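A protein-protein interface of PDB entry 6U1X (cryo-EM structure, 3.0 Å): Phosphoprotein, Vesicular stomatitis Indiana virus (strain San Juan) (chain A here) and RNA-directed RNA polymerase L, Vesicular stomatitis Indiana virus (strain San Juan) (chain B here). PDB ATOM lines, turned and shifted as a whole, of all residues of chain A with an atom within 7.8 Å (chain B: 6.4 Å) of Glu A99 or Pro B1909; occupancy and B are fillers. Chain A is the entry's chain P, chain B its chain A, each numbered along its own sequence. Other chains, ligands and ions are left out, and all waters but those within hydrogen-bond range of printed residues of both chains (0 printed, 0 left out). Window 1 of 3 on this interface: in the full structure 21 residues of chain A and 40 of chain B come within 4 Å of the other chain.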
ATOM      1  N   TYR A  95      25.727   1.745  17.730  1.00  0.00           N
ATOM      2  CA  TYR A  95      26.015   1.618  16.308  1.00  0.00           C
ATOM      3  C   TYR A  95      25.156   2.622  15.550  1.00  0.00           C
ATOM      4  O   TYR A  95      24.337   3.337  16.134  1.00  0.00           O
ATOM      5  CB  TYR A  95      25.764   0.190  15.814  1.00  0.00           C
ATOM      6  CG  TYR A  95      26.827  -0.802  16.219  1.00  0.00           C
ATOM      7  CD1 TYR A  95      27.957  -0.989  15.440  1.00  0.00           C
ATOM      8  CD2 TYR A  95      26.696  -1.558  17.374  1.00  0.00           C
ATOM      9  CE1 TYR A  95      28.931  -1.897  15.803  1.00  0.00           C
ATOM     10  CE2 TYR A  95      27.663  -2.466  17.745  1.00  0.00           C
ATOM     11  CZ  TYR A  95      28.778  -2.632  16.956  1.00  0.00           C
ATOM     12  OH  TYR A  95      29.744  -3.540  17.323  1.00  0.00           O
ATOM     13  N   ALA A  96      25.352   2.674  14.236  1.00  0.00           N
ATOM     14  CA  ALA A  96      24.572   3.565  13.382  1.00  0.00           C
ATOM     15  C   ALA A  96      24.640   3.044  11.958  1.00  0.00           C
ATOM     16  O   ALA A  96      25.725   2.999  11.370  1.00  0.00           O
ATOM     17  CB  ALA A  96      25.099   4.993  13.459  1.00  0.00           C
ATOM     18  N   ASP A  97      23.487   2.656  11.409  1.00  0.00           N
ATOM     19  CA  ASP A  97      23.391   2.177  10.040  1.00  0.00           C
ATOM     20  C   ASP A  97      22.377   2.936   9.201  1.00  0.00           C
ATOM     21  O   ASP A  97      22.474   2.901   7.970  1.00  0.00           O
ATOM     22  CB  ASP A  97      23.021   0.687  10.020  1.00  0.00           C
ATOM     23  CG  ASP A  97      23.962  -0.159  10.857  1.00  0.00           C
ATOM     24  OD1 ASP A  97      25.131   0.246  11.034  1.00  0.00           O
ATOM     25  OD2 ASP A  97      23.535  -1.229  11.338  1.00  0.00           O
ATOM     26  N   GLU A  98      21.413   3.613   9.824  1.00  0.00           N
ATOM     27  CA  GLU A  98      20.457   4.430   9.088  1.00  0.00           C
ATOM     28  C   GLU A  98      21.001   5.814   8.767  1.00  0.00           C
ATOM     29  O   GLU A  98      20.499   6.463   7.843  1.00  0.00           O
ATOM     30  CB  GLU A  98      19.161   4.571   9.889  1.00  0.00           C
ATOM     31  CG  GLU A  98      18.546   3.251  10.325  1.00  0.00           C
ATOM     32  CD  GLU A  98      17.267   3.440  11.115  1.00  0.00           C
ATOM     33  OE1 GLU A  98      16.696   4.549  11.071  1.00  0.00           O
ATOM     34  OE2 GLU A  98      16.833   2.478  11.783  1.00  0.00           O
ATOM     35  N   GLU A  99      22.013   6.278   9.501  1.00  0.00           N
ATOM     36  CA  GLU A  99      22.576   7.605   9.293  1.00  0.00           C
ATOM     37  C   GLU A  99      23.451   7.697   8.051  1.00  0.00           C
ATOM     38  O   GLU A  99      23.940   8.791   7.748  1.00  0.00           O
ATOM     39  CB  GLU A  99      23.389   8.020  10.520  1.00  0.00           C
ATOM     40  CG  GLU A  99      22.571   8.125  11.797  1.00  0.00           C
ATOM     41  CD  GLU A  99      23.359   8.720  12.951  1.00  0.00           C
ATOM     42  OE1 GLU A  99      24.508   9.154  12.729  1.00  0.00           O
ATOM     43  OE2 GLU A  99      22.826   8.755  14.080  1.00  0.00           O
ATOM     44  N   VAL A 100      23.665   6.593   7.333  1.00  0.00           N
ATOM     45  CA  VAL A 100      24.506   6.568   6.145  1.00  0.00           C
ATOM     46  C   VAL A 100      23.750   5.871   5.023  1.00  0.00           C
ATOM     47  O   VAL A 100      22.834   5.080   5.254  1.00  0.00           O
ATOM     48  CB  VAL A 100      25.854   5.865   6.404  1.00  0.00           C
ATOM     49  CG1 VAL A 100      26.733   6.731   7.273  1.00  0.00           C
ATOM     50  CG2 VAL A 100      25.644   4.504   7.061  1.00  0.00           C
ATOM     51  N   ASP A 101      24.151   6.182   3.793  1.00  0.00           N
ATOM     52  CA  ASP A 101      23.530   5.576   2.618  1.00  0.00           C
ATOM     53  C   ASP A 101      24.524   5.672   1.471  1.00  0.00           C
ATOM     54  O   ASP A 101      24.823   6.775   1.004  1.00  0.00           O
ATOM     55  CB  ASP A 101      22.219   6.270   2.274  1.00  0.00           C
ATOM     56  CG  ASP A 101      21.375   5.479   1.293  1.00  0.00           C
ATOM     57  OD1 ASP A 101      21.945   4.754   0.452  1.00  0.00           O
ATOM     58  OD2 ASP A 101      20.133   5.583   1.365  1.00  0.00           O
ATOM     59  N   GLU B1900      30.837  19.842   7.655  1.00  0.00           N
ATOM     60  CA  GLU B1900      30.357  18.474   7.807  1.00  0.00           C
ATOM     61  C   GLU B1900      30.746  17.909   9.166  1.00  0.00           C
ATOM     62  O   GLU B1900      29.893  17.438   9.926  1.00  0.00           O
ATOM     63  CB  GLU B1900      30.905  17.607   6.675  1.00  0.00           C
ATOM     64  CG  GLU B1900      30.396  16.181   6.673  1.00  0.00           C
ATOM     65  CD  GLU B1900      30.784  15.425   5.419  1.00  0.00           C
ATOM     66  OE1 GLU B1900      31.374  16.041   4.507  1.00  0.00           O
ATOM     67  OE2 GLU B1900      30.503  14.211   5.348  1.00  0.00           O
ATOM     68  N   LEU B1903      28.944  19.887  12.159  1.00  0.00           N
ATOM     69  CA  LEU B1903      27.596  19.372  12.364  1.00  0.00           C
ATOM     70  C   LEU B1903      27.634  17.973  12.961  1.00  0.00           C
ATOM     71  O   LEU B1903      26.832  17.643  13.841  1.00  0.00           O
ATOM     72  CB  LEU B1903      26.831  19.367  11.042  1.00  0.00           C
ATOM     73  CG  LEU B1903      26.604  20.720  10.370  1.00  0.00           C
ATOM     74  CD1 LEU B1903      26.143  20.529   8.948  1.00  0.00           C
ATOM     75  CD2 LEU B1903      25.591  21.536  11.137  1.00  0.00           C
ATOM     76  N   GLN B1904      28.573  17.140  12.509  1.00  0.00           N
ATOM     77  CA  GLN B1904      28.689  15.794  13.051  1.00  0.00           C
ATOM     78  C   GLN B1904      29.043  15.813  14.532  1.00  0.00           C
ATOM     79  O   GLN B1904      28.708  14.873  15.262  1.00  0.00           O
ATOM     80  CB  GLN B1904      29.731  15.009  12.256  1.00  0.00           C
ATOM     81  CG  GLN B1904      29.829  13.544  12.614  1.00  0.00           C
ATOM     82  CD  GLN B1904      30.737  12.781  11.674  1.00  0.00           C
ATOM     83  OE1 GLN B1904      31.188  13.314  10.660  1.00  0.00           O
ATOM     84  NE2 GLN B1904      31.011  11.527  12.004  1.00  0.00           N
ATOM     85  N   GLY B1907      25.608  16.623  17.347  1.00  0.00           N
ATOM     86  CA  GLY B1907      24.489  15.705  17.352  1.00  0.00           C
ATOM     87  C   GLY B1907      23.931  15.323  15.999  1.00  0.00           C
ATOM     88  O   GLY B1907      23.125  14.387  15.929  1.00  0.00           O
ATOM     89  N   VAL B1908      24.322  15.997  14.923  1.00  0.00           N
ATOM     90  CA  VAL B1908      23.720  15.772  13.612  1.00  0.00           C
ATOM     91  C   VAL B1908      24.286  14.485  13.021  1.00  0.00           C
ATOM     92  O   VAL B1908      25.465  14.176  13.247  1.00  0.00           O
ATOM     93  CB  VAL B1908      23.959  16.967  12.679  1.00  0.00           C
ATOM     94  CG1 VAL B1908      23.191  16.794  11.391  1.00  0.00           C
ATOM     95  CG2 VAL B1908      23.549  18.253  13.365  1.00  0.00           C
ATOM     96  N   PRO B1909      23.501  13.698  12.264  1.00  0.00           N
ATOM     97  CA  PRO B1909      24.060  12.478  11.666  1.00  0.00           C
ATOM     98  C   PRO B1909      25.118  12.755  10.613  1.00  0.00           C
ATOM     99  O   PRO B1909      25.409  13.911  10.289  1.00  0.00           O
ATOM    100  CB  PRO B1909      22.833  11.794  11.052  1.00  0.00           C
ATOM    101  CG  PRO B1909      21.683  12.350  11.775  1.00  0.00           C
ATOM    102  CD  PRO B1909      22.043  13.761  12.067  1.00  0.00           C
ATOM    103  N   THR B1910      25.699  11.685  10.070  1.00  0.00           N
ATOM    104  CA  THR B1910      26.806  11.808   9.127  1.00  0.00           C
ATOM    105  C   THR B1910      26.310  12.179   7.734  1.00  0.00           C
ATOM    106  O   THR B1910      26.737  13.185   7.159  1.00  0.00           O
ATOM    107  CB  THR B1910      27.591  10.497   9.073  1.00  0.00           C
ATOM    108  OG1 THR B1910      26.778   9.485   8.470  1.00  0.00           O
ATOM    109  CG2 THR B1910      27.991  10.050  10.469  1.00  0.00           C
ATOM    110  N   GLY B1911      25.413  11.367   7.172  1.00  0.00           N
ATOM    111  CA  GLY B1911      24.923  11.639   5.833  1.00  0.00           C
ATOM    112  C   GLY B1911      24.096  12.905   5.753  1.00  0.00           C
ATOM    113  O   GLY B1911      24.137  13.618   4.744  1.00  0.00           O
ATOM    114  N   VAL B1912      23.334  13.203   6.806  1.00  0.00           N
ATOM    115  CA  VAL B1912      22.561  14.440   6.827  1.00  0.00           C
ATOM    116  C   VAL B1912      23.495  15.640   6.789  1.00  0.00           C
ATOM    117  O   VAL B1912      23.256  16.610   6.061  1.00  0.00           O
ATOM    118  CB  VAL B1912      21.644  14.478   8.063  1.00  0.00           C
ATOM    119  CG1 VAL B1912      20.798  15.736   8.052  1.00  0.00           C
ATOM    120  CG2 VAL B1912      20.766  13.238   8.115  1.00  0.00           C
ATOM    121  N   SER B1913      24.578  15.589   7.565  1.00  0.00           N
ATOM    122  CA  SER B1913      25.556  16.670   7.543  1.00  0.00           C
ATOM    123  C   SER B1913      26.240  16.761   6.187  1.00  0.00           C
ATOM    124  O   SER B1913      26.500  17.862   5.690  1.00  0.00           O
ATOM    125  CB  SER B1913      26.584  16.460   8.651  1.00  0.00           C
ATOM    126  OG  SER B1913      27.262  15.229   8.490  1.00  0.00           O
ATOM    127  N   HIS B1914      26.538  15.614   5.577  1.00  0.00           N
ATOM    128  CA  HIS B1914      27.120  15.601   4.239  1.00  0.00           C
ATOM    129  C   HIS B1914      26.226  16.341   3.253  1.00  0.00           C
ATOM    130  O   HIS B1914      26.684  17.221   2.513  1.00  0.00           O
ATOM    131  CB  HIS B1914      27.338  14.154   3.793  1.00  0.00           C
ATOM    132  CG  HIS B1914      28.200  14.011   2.578  1.00  0.00           C
ATOM    133  ND1 HIS B1914      27.846  14.519   1.347  1.00  0.00           N
ATOM    134  CD2 HIS B1914      29.393  13.395   2.402  1.00  0.00           C
ATOM    135  CE1 HIS B1914      28.789  14.232   0.467  1.00  0.00           C
ATOM    136  NE2 HIS B1914      29.737  13.550   1.082  1.00  0.00           N
ATOM    137  N   TYR B1941      17.962  17.585  16.235  1.00  0.00           N
ATOM    138  CA  TYR B1941      18.644  16.348  16.586  1.00  0.00           C
ATOM    139  C   TYR B1941      19.186  16.350  18.005  1.00  0.00           C
ATOM    140  O   TYR B1941      19.596  15.289  18.489  1.00  0.00           O
ATOM    141  CB  TYR B1941      19.786  16.076  15.606  1.00  0.00           C
ATOM    142  CG  TYR B1941      19.334  15.422  14.324  1.00  0.00           C
ATOM    143  CD1 TYR B1941      19.137  14.053  14.257  1.00  0.00           C
ATOM    144  CD2 TYR B1941      19.099  16.173  13.184  1.00  0.00           C
ATOM    145  CE1 TYR B1941      18.723  13.449  13.092  1.00  0.00           C
ATOM    146  CE2 TYR B1941      18.684  15.578  12.014  1.00  0.00           C
ATOM    147  CZ  TYR B1941      18.497  14.217  11.973  1.00  0.00           C
ATOM    148  OH  TYR B1941      18.083  13.620  10.806  1.00  0.00           O
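The side-chain hydroxyl (OG1) of Thr B1910 sits at hydrogen-bond distance from the backbone carbonyl oxygen (O) of Glu A99 (3.0 Å). N of Gly B1911 sits at hydrogen-bond distance from O of Glu A99 (3.0 Å).
The side-chain hydroxyl of Ser B1913 is in hydrogen-bond range of the backbone carbonyl oxygen of Pro B1909 (2.9 Å). The side-chain hydroxyl (OG) of Ser B1913 is in hydrogen-bond range of the backbone carbonyl oxygen (O) of Thr B1910 (2.5 Å).
Among the printed residues, merely in contact across the chains: Val A100 with Thr B1910 and Glu A99 with Pro B1909.
Glu A99 touches just these residues of chain B: Pro B1909 (3.5 Å), Thr B1910 (3.0 Å) and Gly B1911 (3.0 Å). Pro B1909 touches one residue of chain A. Of the printed residues of chain B, Val A100 touches Thr B1910 (3.0 Å). Printed residues of chain A within 4 Å of Gly B1911: Glu A99. Glu A98 touches none of the printed residues of chain B. Tyr A95 touches none of the printed residues of chain B. The nearest residue of chain B that does not touch Glu A99 is Val B1912 (4.6 Å). The nearest residue of chain A that does not touch Pro B1909 is Val A100 (6.4 Å).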
